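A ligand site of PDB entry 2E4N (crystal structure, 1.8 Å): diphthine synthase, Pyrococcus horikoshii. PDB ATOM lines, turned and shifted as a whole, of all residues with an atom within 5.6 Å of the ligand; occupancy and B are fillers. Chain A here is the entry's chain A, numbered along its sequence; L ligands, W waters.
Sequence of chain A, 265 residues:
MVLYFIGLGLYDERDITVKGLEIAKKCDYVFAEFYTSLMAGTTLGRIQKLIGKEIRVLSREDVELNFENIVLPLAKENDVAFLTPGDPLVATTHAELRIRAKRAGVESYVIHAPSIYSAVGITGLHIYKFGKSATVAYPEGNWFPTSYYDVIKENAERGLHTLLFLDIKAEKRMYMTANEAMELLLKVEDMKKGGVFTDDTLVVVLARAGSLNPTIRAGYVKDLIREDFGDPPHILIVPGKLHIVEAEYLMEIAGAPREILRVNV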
ATOM      1  N   LEU A  10      -3.016  27.284 -25.620  1.00  0.00           N
ATOM      2  CA  LEU A  10      -2.228  26.172 -25.097  1.00  0.00           C
ATOM      3  C   LEU A  10      -1.051  25.538 -25.816  1.00  0.00           C
ATOM      4  O   LEU A  10       0.003  25.310 -25.222  1.00  0.00           O
ATOM      5  CB  LEU A  10      -3.181  25.032 -24.748  1.00  0.00           C
ATOM      6  CG  LEU A  10      -4.371  25.309 -23.830  1.00  0.00           C
ATOM      7  CD1 LEU A  10      -5.398  24.209 -23.994  1.00  0.00           C
ATOM      8  CD2 LEU A  10      -3.907  25.398 -22.382  1.00  0.00           C
ATOM      9  N   TYR A  11      -1.243  25.218 -27.095  1.00  0.00           N
ATOM     10  CA  TYR A  11      -0.234  24.463 -27.817  1.00  0.00           C
ATOM     11  C   TYR A  11       0.290  25.017 -29.144  1.00  0.00           C
ATOM     12  O   TYR A  11       1.502  25.036 -29.378  1.00  0.00           O
ATOM     13  CB  TYR A  11      -0.809  23.059 -28.031  1.00  0.00           C
ATOM     14  CG  TYR A  11       0.103  22.057 -28.699  1.00  0.00           C
ATOM     15  CD1 TYR A  11       1.192  21.514 -28.021  1.00  0.00           C
ATOM     16  CD2 TYR A  11      -0.137  21.641 -30.006  1.00  0.00           C
ATOM     17  CE1 TYR A  11       2.023  20.565 -28.638  1.00  0.00           C
ATOM     18  CE2 TYR A  11       0.683  20.703 -30.631  1.00  0.00           C
ATOM     19  CZ  TYR A  11       1.764  20.170 -29.941  1.00  0.00           C
ATOM     20  OH  TYR A  11       2.577  19.242 -30.545  1.00  0.00           O
ATOM     21  N   THR A  36       6.723  33.118 -20.317  1.00  0.00           N
ATOM     22  CA  THR A  36       5.797  32.675 -19.258  1.00  0.00           C
ATOM     23  C   THR A  36       5.296  31.246 -19.442  1.00  0.00           C
ATOM     24  O   THR A  36       4.791  30.633 -18.493  1.00  0.00           O
ATOM     25  CB  THR A  36       4.567  33.602 -19.147  1.00  0.00           C
ATOM     26  OG1 THR A  36       3.924  33.728 -20.422  1.00  0.00           O
ATOM     27  CG2 THR A  36       4.986  34.986 -18.643  1.00  0.00           C
ATOM     28  N   SER A  37       5.425  30.706 -20.649  1.00  0.00           N
ATOM     29  CA  SER A  37       4.968  29.346 -20.906  1.00  0.00           C
ATOM     30  C   SER A  37       5.540  28.865 -22.228  1.00  0.00           C
ATOM     31  O   SER A  37       6.225  29.611 -22.931  1.00  0.00           O
ATOM     32  CB  SER A  37       3.436  29.293 -20.945  1.00  0.00           C
ATOM     33  OG  SER A  37       2.992  27.957 -21.031  1.00  0.00           O
ATOM     34  N   LEU A  38       5.259  27.609 -22.573  1.00  0.00           N
ATOM     35  CA  LEU A  38       5.756  27.029 -23.809  1.00  0.00           C
ATOM     36  C   LEU A  38       4.635  26.518 -24.705  1.00  0.00           C
ATOM     37  O   LEU A  38       3.812  25.709 -24.268  1.00  0.00           O
ATOM     38  CB  LEU A  38       6.725  25.883 -23.512  1.00  0.00           C
ATOM     39  CG  LEU A  38       7.226  25.061 -24.697  1.00  0.00           C
ATOM     40  CD1 LEU A  38       8.105  25.932 -25.592  1.00  0.00           C
ATOM     41  CD2 LEU A  38       7.995  23.840 -24.196  1.00  0.00           C
ATOM     42  N   PRO A  85       1.499  33.308 -24.418  1.00  0.00           N
ATOM     43  CA  PRO A  85       1.021  31.925 -24.521  1.00  0.00           C
ATOM     44  C   PRO A  85      -0.162  31.830 -23.558  1.00  0.00           C
ATOM     45  O   PRO A  85      -0.285  32.640 -22.643  1.00  0.00           O
ATOM     46  CB  PRO A  85       2.203  31.102 -24.027  1.00  0.00           C
ATOM     47  CG  PRO A  85       3.380  31.957 -24.326  1.00  0.00           C
ATOM     48  CD  PRO A  85       2.912  33.345 -23.970  1.00  0.00           C
ATOM     49  N   GLY A  86      -1.027  30.832 -23.759  1.00  0.00           N
ATOM     50  CA  GLY A  86      -2.186  30.659 -22.892  1.00  0.00           C
ATOM     51  C   GLY A  86      -2.997  31.922 -22.720  1.00  0.00           C
ATOM     52  O   GLY A  86      -3.193  32.674 -23.675  1.00  0.00           O
ATOM     53  N   ASP A  87      -3.505  32.152 -21.507  1.00  0.00           N
ATOM     54  CA  ASP A  87      -4.262  33.357 -21.203  1.00  0.00           C
ATOM     55  C   ASP A  87      -3.212  34.324 -20.653  1.00  0.00           C
ATOM     56  O   ASP A  87      -2.416  33.942 -19.801  1.00  0.00           O
ATOM     57  CB  ASP A  87      -5.344  33.064 -20.159  1.00  0.00           C
ATOM     58  CG  ASP A  87      -6.176  34.282 -19.814  1.00  0.00           C
ATOM     59  OD1 ASP A  87      -5.659  35.215 -19.158  1.00  0.00           O
ATOM     60  OD2 ASP A  87      -7.366  34.311 -20.207  1.00  0.00           O
ATOM     61  N   PRO A  88      -3.200  35.570 -21.131  1.00  0.00           N
ATOM     62  CA  PRO A  88      -2.212  36.553 -20.674  1.00  0.00           C
ATOM     63  C   PRO A  88      -2.124  36.882 -19.190  1.00  0.00           C
ATOM     64  O   PRO A  88      -1.052  37.248 -18.696  1.00  0.00           O
ATOM     65  CB  PRO A  88      -2.538  37.790 -21.513  1.00  0.00           C
ATOM     66  CG  PRO A  88      -4.017  37.669 -21.733  1.00  0.00           C
ATOM     67  CD  PRO A  88      -4.183  36.195 -22.041  1.00  0.00           C
ATOM     68  N   LEU A  89      -3.229  36.731 -18.460  1.00  0.00           N
ATOM     69  CA  LEU A  89      -3.250  37.088 -17.041  1.00  0.00           C
ATOM     70  C   LEU A  89      -3.150  35.938 -16.039  1.00  0.00           C
ATOM     71  O   LEU A  89      -3.052  36.186 -14.832  1.00  0.00           O
ATOM     72  CB  LEU A  89      -4.500  37.899 -16.730  1.00  0.00           C
ATOM     73  CG  LEU A  89      -4.823  39.069 -17.663  1.00  0.00           C
ATOM     74  CD1 LEU A  89      -6.110  39.747 -17.191  1.00  0.00           C
ATOM     75  CD2 LEU A  89      -3.662  40.067 -17.671  1.00  0.00           C
ATOM     76  N   VAL A  90      -3.176  34.703 -16.527  1.00  0.00           N
ATOM     77  CA  VAL A  90      -3.133  33.530 -15.650  1.00  0.00           C
ATOM     78  C   VAL A  90      -1.726  33.070 -15.282  1.00  0.00           C
ATOM     79  O   VAL A  90      -0.938  32.672 -16.133  1.00  0.00           O
ATOM     80  CB  VAL A  90      -3.883  32.350 -16.296  1.00  0.00           C
ATOM     81  CG1 VAL A  90      -3.739  31.083 -15.456  1.00  0.00           C
ATOM     82  CG2 VAL A  90      -5.359  32.718 -16.458  1.00  0.00           C
ATOM     83  N   ALA A  91      -1.426  33.102 -13.987  1.00  0.00           N
ATOM     84  CA  ALA A  91      -0.120  32.673 -13.473  1.00  0.00           C
ATOM     85  C   ALA A  91       1.023  33.470 -14.092  1.00  0.00           C
ATOM     86  O   ALA A  91       2.087  32.929 -14.389  1.00  0.00           O
ATOM     87  CB  ALA A  91       0.074  31.176 -13.717  1.00  0.00           C
ATOM     88  N   THR A  92       0.776  34.754 -14.324  1.00  0.00           N
ATOM     89  CA  THR A  92       1.743  35.745 -14.741  1.00  0.00           C
ATOM     90  C   THR A  92       1.540  37.003 -13.921  1.00  0.00           C
ATOM     91  O   THR A  92       0.630  37.109 -13.115  1.00  0.00           O
ATOM     92  CB  THR A  92       1.516  36.065 -16.234  1.00  0.00           C
ATOM     93  OG1 THR A  92       0.339  36.857 -16.366  1.00  0.00           O
ATOM     94  CG2 THR A  92       1.356  34.777 -17.040  1.00  0.00           C
ATOM     95  N   PRO A 114      -7.583  29.774 -24.379  1.00  0.00           N
ATOM     96  CA  PRO A 114      -7.569  28.603 -23.488  1.00  0.00           C
ATOM     97  C   PRO A 114      -6.317  28.586 -22.619  1.00  0.00           C
ATOM     98  O   PRO A 114      -5.207  28.790 -23.095  1.00  0.00           O
ATOM     99  CB  PRO A 114      -7.655  27.416 -24.461  1.00  0.00           C
ATOM    100  CG  PRO A 114      -7.138  27.970 -25.766  1.00  0.00           C
ATOM    101  CD  PRO A 114      -7.696  29.364 -25.793  1.00  0.00           C
ATOM    102  N   SER A 115      -6.535  28.357 -21.319  1.00  0.00           N
ATOM    103  CA  SER A 115      -5.485  28.357 -20.302  1.00  0.00           C
ATOM    104  C   SER A 115      -5.285  26.973 -19.685  1.00  0.00           C
ATOM    105  O   SER A 115      -6.222  26.201 -19.596  1.00  0.00           O
ATOM    106  CB  SER A 115      -5.856  29.355 -19.198  1.00  0.00           C
ATOM    107  OG  SER A 115      -5.011  29.222 -18.069  1.00  0.00           O
ATOM    108  N   ILE A 116      -4.072  26.682 -19.245  1.00  0.00           N
ATOM    109  CA  ILE A 116      -3.825  25.396 -18.620  1.00  0.00           C
ATOM    110  C   ILE A 116      -4.667  25.282 -17.347  1.00  0.00           C
ATOM    111  O   ILE A 116      -5.010  24.185 -16.912  1.00  0.00           O
ATOM    112  CB  ILE A 116      -2.327  25.201 -18.273  1.00  0.00           C
ATOM    113  CG1 ILE A 116      -2.098  23.760 -17.802  1.00  0.00           C
ATOM    114  CG2 ILE A 116      -1.896  26.196 -17.210  1.00  0.00           C
ATOM    115  CD1 ILE A 116      -2.419  22.709 -18.851  1.00  0.00           C
ATOM    116  N   TYR A 117      -5.016  26.425 -16.754  1.00  0.00           N
ATOM    117  CA  TYR A 117      -5.786  26.420 -15.527  1.00  0.00           C
ATOM    118  C   TYR A 117      -7.154  25.739 -15.682  1.00  0.00           C
ATOM    119  O   TYR A 117      -7.634  25.095 -14.758  1.00  0.00           O
ATOM    120  CB  TYR A 117      -5.946  27.844 -14.987  1.00  0.00           C
ATOM    121  CG  TYR A 117      -6.435  27.887 -13.552  1.00  0.00           C
ATOM    122  CD1 TYR A 117      -5.614  27.487 -12.501  1.00  0.00           C
ATOM    123  CD2 TYR A 117      -7.738  28.321 -13.259  1.00  0.00           C
ATOM    124  CE1 TYR A 117      -6.068  27.511 -11.182  1.00  0.00           C
ATOM    125  CE2 TYR A 117      -8.202  28.345 -11.938  1.00  0.00           C
ATOM    126  CZ  TYR A 117      -7.363  27.945 -10.910  1.00  0.00           C
ATOM    127  OH  TYR A 117      -7.822  27.970  -9.620  1.00  0.00           O
ATOM    128  N   LEU A 164      -0.067  22.043  -9.824  1.00  0.00           N
ATOM    129  CA  LEU A 164       1.306  22.494  -9.689  1.00  0.00           C
ATOM    130  C   LEU A 164       1.883  22.934 -11.026  1.00  0.00           C
ATOM    131  O   LEU A 164       2.173  22.093 -11.883  1.00  0.00           O
ATOM    132  CB  LEU A 164       2.190  21.374  -9.118  1.00  0.00           C
ATOM    133  CG  LEU A 164       1.844  20.908  -7.700  1.00  0.00           C
ATOM    134  CD1 LEU A 164       2.538  19.578  -7.426  1.00  0.00           C
ATOM    135  CD2 LEU A 164       2.261  21.965  -6.693  1.00  0.00           C
ATOM    136  N   PHE A 165       2.007  24.236 -11.214  1.00  0.00           N
ATOM    137  CA  PHE A 165       2.605  24.782 -12.429  1.00  0.00           C
ATOM    138  C   PHE A 165       4.065  24.376 -12.297  1.00  0.00           C
ATOM    139  O   PHE A 165       4.581  24.322 -11.174  1.00  0.00           O
ATOM    140  CB  PHE A 165       2.523  26.310 -12.430  1.00  0.00           C
ATOM    141  CG  PHE A 165       1.115  26.852 -12.523  1.00  0.00           C
ATOM    142  CD1 PHE A 165       0.445  26.888 -13.738  1.00  0.00           C
ATOM    143  CD2 PHE A 165       0.468  27.334 -11.393  1.00  0.00           C
ATOM    144  CE1 PHE A 165      -0.864  27.395 -13.834  1.00  0.00           C
ATOM    145  CE2 PHE A 165      -0.838  27.850 -11.470  1.00  0.00           C
ATOM    146  CZ  PHE A 165      -1.500  27.875 -12.696  1.00  0.00           C
ATOM    147  N   LEU A 166       4.745  24.072 -13.404  1.00  0.00           N
ATOM    148  CA  LEU A 166       6.150  23.691 -13.315  1.00  0.00           C
ATOM    149  C   LEU A 166       7.051  24.809 -13.820  1.00  0.00           C
ATOM    150  O   LEU A 166       6.659  25.609 -14.677  1.00  0.00           O
ATOM    151  CB  LEU A 166       6.387  22.379 -14.081  1.00  0.00           C
ATOM    152  CG  LEU A 166       5.494  21.230 -13.578  1.00  0.00           C
ATOM    153  CD1 LEU A 166       5.895  19.937 -14.254  1.00  0.00           C
ATOM    154  CD2 LEU A 166       5.614  21.105 -12.055  1.00  0.00           C
ATOM    155  N   ASP A 167       8.248  24.885 -13.263  1.00  0.00           N
ATOM    156  CA  ASP A 167       9.189  25.945 -13.593  1.00  0.00           C
ATOM    157  C   ASP A 167       9.639  25.986 -15.051  1.00  0.00           C
ATOM    158  O   ASP A 167       9.543  25.002 -15.793  1.00  0.00           O
ATOM    159  CB  ASP A 167      10.421  25.838 -12.685  1.00  0.00           C
ATOM    160  CG  ASP A 167      11.063  27.196 -12.401  1.00  0.00           C
ATOM    161  OD1 ASP A 167      10.598  28.211 -12.969  1.00  0.00           O
ATOM    162  OD2 ASP A 167      12.034  27.227 -11.615  1.00  0.00           O
ATOM    163  N   ILE A 168      10.113  27.164 -15.449  1.00  0.00           N
ATOM    164  CA  ILE A 168      10.586  27.391 -16.802  1.00  0.00           C
ATOM    165  C   ILE A 168      11.717  28.421 -16.825  1.00  0.00           C
ATOM    166  O   ILE A 168      11.645  29.456 -16.151  1.00  0.00           O
ATOM    167  CB  ILE A 168       9.431  27.865 -17.727  1.00  0.00           C
ATOM    168  CG1 ILE A 168       9.978  28.239 -19.113  1.00  0.00           C
ATOM    169  CG2 ILE A 168       8.714  29.048 -17.106  1.00  0.00           C
ATOM    170  CD1 ILE A 168       8.885  28.443 -20.157  1.00  0.00           C
ATOM    171  N   LEU A 206      -0.257  15.904 -16.897  1.00  0.00           N
ATOM    172  CA  LEU A 206      -0.887  16.368 -18.130  1.00  0.00           C
ATOM    173  C   LEU A 206       0.228  17.042 -18.912  1.00  0.00           C
ATOM    174  O   LEU A 206       0.812  18.017 -18.454  1.00  0.00           O
ATOM    175  CB  LEU A 206      -2.009  17.364 -17.838  1.00  0.00           C
ATOM    176  CG  LEU A 206      -2.638  18.038 -19.064  1.00  0.00           C
ATOM    177  CD1 LEU A 206      -3.170  16.976 -20.026  1.00  0.00           C
ATOM    178  CD2 LEU A 206      -3.756  18.969 -18.634  1.00  0.00           C
ATOM    179  N   ALA A 207       0.524  16.491 -20.080  1.00  0.00           N
ATOM    180  CA  ALA A 207       1.584  17.030 -20.920  1.00  0.00           C
ATOM    181  C   ALA A 207       1.059  17.493 -22.278  1.00  0.00           C
ATOM    182  O   ALA A 207       0.320  16.773 -22.949  1.00  0.00           O
ATOM    183  CB  ALA A 207       2.665  15.984 -21.118  1.00  0.00           C
ATOM    184  N   ARG A 208       1.455  18.705 -22.665  1.00  0.00           N
ATOM    185  CA  ARG A 208       1.077  19.278 -23.947  1.00  0.00           C
ATOM    186  C   ARG A 208      -0.426  19.398 -24.145  1.00  0.00           C
ATOM    187  O   ARG A 208      -0.963  18.969 -25.163  1.00  0.00           O
ATOM    188  CB  ARG A 208       1.716  18.466 -25.088  1.00  0.00           C
ATOM    189  CG  ARG A 208       3.240  18.358 -24.973  1.00  0.00           C
ATOM    190  CD  ARG A 208       3.831  17.488 -26.071  1.00  0.00           C
ATOM    191  NE  ARG A 208       3.157  16.195 -26.156  1.00  0.00           N
ATOM    192  CZ  ARG A 208       3.256  15.229 -25.237  1.00  0.00           C
ATOM    193  NH1 ARG A 208       4.020  15.393 -24.158  1.00  0.00           N
ATOM    194  NH2 ARG A 208       2.572  14.110 -25.395  1.00  0.00           N
ATOM    195  N   ALA A 209      -1.109  19.966 -23.169  1.00  0.00           N
ATOM    196  CA  ALA A 209      -2.548  20.161 -23.291  1.00  0.00           C
ATOM    197  C   ALA A 209      -2.728  21.071 -24.504  1.00  0.00           C
ATOM    198  O   ALA A 209      -1.855  21.893 -24.795  1.00  0.00           O
ATOM    199  CB  ALA A 209      -3.098  20.833 -22.035  1.00  0.00           C
ATOM    200  N   GLY A 210      -3.838  20.914 -25.217  1.00  0.00           N
ATOM    201  CA  GLY A 210      -4.067  21.736 -26.387  1.00  0.00           C
ATOM    202  C   GLY A 210      -3.715  20.964 -27.651  1.00  0.00           C
ATOM    203  O   GLY A 210      -4.243  21.248 -28.723  1.00  0.00           O
ATOM    204  N   PRO A 233       5.421  21.378 -22.582  1.00  0.00           N
ATOM    205  CA  PRO A 233       5.286  21.600 -21.134  1.00  0.00           C
ATOM    206  C   PRO A 233       4.456  20.541 -20.413  1.00  0.00           C
ATOM    207  O   PRO A 233       3.616  19.866 -21.019  1.00  0.00           O
ATOM    208  CB  PRO A 233       4.659  22.986 -21.071  1.00  0.00           C
ATOM    209  CG  PRO A 233       3.719  22.944 -22.235  1.00  0.00           C
ATOM    210  CD  PRO A 233       4.565  22.310 -23.325  1.00  0.00           C
ATOM    211  N   HIS A 234       4.698  20.407 -19.108  1.00  0.00           N
ATOM    212  CA  HIS A 234       3.993  19.467 -18.247  1.00  0.00           C
ATOM    213  C   HIS A 234       3.451  20.200 -17.031  1.00  0.00           C
ATOM    214  O   HIS A 234       3.957  21.253 -16.661  1.00  0.00           O
ATOM    215  CB  HIS A 234       4.953  18.423 -17.663  1.00  0.00           C
ATOM    216  CG  HIS A 234       5.647  17.544 -18.663  1.00  0.00           C
ATOM    217  ND1 HIS A 234       6.566  16.589 -18.282  1.00  0.00           N
ATOM    218  CD2 HIS A 234       5.541  17.462 -20.004  1.00  0.00           C
ATOM    219  CE1 HIS A 234       6.989  15.948 -19.359  1.00  0.00           C
ATOM    220  NE2 HIS A 234       6.384  16.456 -20.422  1.00  0.00           N
ATOM    221  N   ILE A 235       2.401  19.659 -16.424  1.00  0.00           N
ATOM    222  CA  ILE A 235       1.893  20.178 -15.169  1.00  0.00           C
ATOM    223  C   ILE A 235       1.723  18.919 -14.339  1.00  0.00           C
ATOM    224  O   ILE A 235       1.516  17.835 -14.879  1.00  0.00           O
ATOM    225  CB  ILE A 235       0.497  20.880 -15.237  1.00  0.00           C
ATOM    226  CG1 ILE A 235      -0.519  19.997 -15.949  1.00  0.00           C
ATOM    227  CG2 ILE A 235       0.637  22.234 -15.868  1.00  0.00           C
ATOM    228  CD1 ILE A 235      -1.959  20.420 -15.699  1.00  0.00           C
HETATM  229  N1  LIG L   1      -0.768  32.062 -18.721  1.00  0.00           N
HETATM  230  C1  LIG L   1      -0.488  30.580 -18.934  1.00  0.00           C
HETATM  231  C2  LIG L   1       0.237  29.893 -17.812  1.00  0.00           C
HETATM  232  C3  LIG L   1       1.599  30.436 -17.409  1.00  0.00           C
HETATM  233  S1  LIG L   1       2.357  29.244 -16.220  1.00  0.00           S
HETATM  234  C4  LIG L   1      -1.884  29.885 -19.218  1.00  0.00           C
HETATM  235  O1  LIG L   1      -2.914  30.593 -19.191  1.00  0.00           O
HETATM  236  O2  LIG L   1      -1.880  28.610 -19.459  1.00  0.00           O
HETATM  237  C5  LIG L   1       3.241  28.238 -17.339  1.00  0.00           C
HETATM  238  C6  LIG L   1       3.272  26.747 -16.816  1.00  0.00           C
HETATM  239  O3  LIG L   1       1.916  26.215 -16.937  1.00  0.00           O
HETATM  240  C7  LIG L   1       4.154  25.830 -17.589  1.00  0.00           C
HETATM  241  O4  LIG L   1       5.484  25.870 -17.080  1.00  0.00           O
HETATM  242  C8  LIG L   1       3.422  24.482 -17.406  1.00  0.00           C
HETATM  243  O5  LIG L   1       3.752  23.864 -16.161  1.00  0.00           O
HETATM  244  C9  LIG L   1       1.930  24.850 -17.536  1.00  0.00           C
HETATM  245  N2  LIG L   1       1.443  24.857 -18.805  1.00  0.00           N
HETATM  246  C10 LIG L   1       1.125  25.856 -19.715  1.00  0.00           C
HETATM  247  N3  LIG L   1       0.665  25.446 -20.852  1.00  0.00           N
HETATM  248  C11 LIG L   1       0.657  24.030 -20.735  1.00  0.00           C
HETATM  249  C12 LIG L   1       0.252  22.999 -21.661  1.00  0.00           C
HETATM  250  N4  LIG L   1      -0.229  23.236 -22.902  1.00  0.00           N
HETATM  251  N5  LIG L   1       0.378  21.715 -21.192  1.00  0.00           N
HETATM  252  C13 LIG L   1       0.857  21.419 -19.943  1.00  0.00           C
HETATM  253  N6  LIG L   1       1.255  22.370 -19.038  1.00  0.00           N
HETATM  254  C14 LIG L   1       1.120  23.654 -19.496  1.00  0.00           C
HETATM  255  O   HOH W   1       1.529  27.650 -23.329  1.00  0.00           O
HETATM  256  O   HOH W   2       7.715  24.435 -18.075  1.00  0.00           O
HETATM  257  O   HOH W   3       1.347  32.925 -20.277  1.00  0.00           O
HETATM  258  O   HOH W   4      -0.816  27.546 -21.905  1.00  0.00           O
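The backbone carbonyl oxygen (O) of Leu 10 sits at hydrogen-bond distance from a nitrogen (N4) of the ligand (3.1 Å). The backbone carbonyl oxygen (O) of Val 90 sits at hydrogen-bond distance from a nitrogen (N1) of the ligand (2.7 Å). O of His 234 sits at hydrogen-bond distance from O5 of the ligand, at 2.7 Å. A nitrogen (N3) of the ligand sits close to the side-chain hydroxyl (OG) of Ser 37, at 3.4 Å. A nitrogen (N5) of the ligand is in hydrogen-bond range of the backbone NH of Ala 209 (3.0 Å). An oxygen (O2) of the ligand lies within hydrogen-bond range of the backbone NH of Ile 116, 2.9 Å away. O of Ala 209 lies within hydrogen-bond range of N4 of the ligand (2.8 Å). The backbone NH of Leu 166 sits at hydrogen-bond distance from an oxygen (O5) of the ligand, at 2.9 Å. The backbone NH (N) of Asp 87 sits at hydrogen-bond distance from an oxygen (O1) of the ligand, at 2.9 Å. An oxygen (O1) of the ligand sits at hydrogen-bond distance from the side-chain hydroxyl of Ser 115 (2.7 Å). O of Asp 87 sits at hydrogen-bond distance from N1 of the ligand (2.7 Å). An oxygen (O4) of the ligand is in hydrogen-bond range of the backbone carbonyl oxygen of Leu 166 (2.7 Å).
The backbone carbonyl oxygen of Thr 36 sits close to a sulfur (S1) of the ligand. Residues that only touch the ligand: Ile 235 (3.2 Å), Pro 233 (3.3 Å), Arg 208 (3.5 Å), Phe 165 (3.6 Å), Leu 206 (3.7 Å), Gly 86 (3.8 Å), Thr 92 (3.8 Å), Ala 91 (3.9 Å) and Pro 85 (3.99 Å). Of the 30 residues printed, 19 come within 4 Å of the ligand. The nearest printed residue that does not touch the ligand is Asp 167 (4.3 Å).
Water W3 lies within hydrogen-bond range of the side-chain hydroxyl of Thr 36, a nitrogen (N1) of the ligand and the backbone carbonyl oxygen of Pro 85. Water W2 bridges O4 of the ligand (2.8 Å) and O of Asp 167 (3.0 Å).
OG1 of Thr 92 sits at hydrogen-bond distance from O of Pro 88 (2.7 Å). The backbone NH of Tyr 117 lies close to the side-chain hydroxyl of Ser 115 (3.1 Å). N of Arg 208 is in hydrogen-bond range of O of Pro 233. O of Leu 206 sits at hydrogen-bond distance from N of Ile 235 (3.1 Å). The backbone NH (N) of Leu 89 sits at hydrogen-bond distance from the side-chain carboxylate (OD1) of Asp 87 (2.9 Å).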
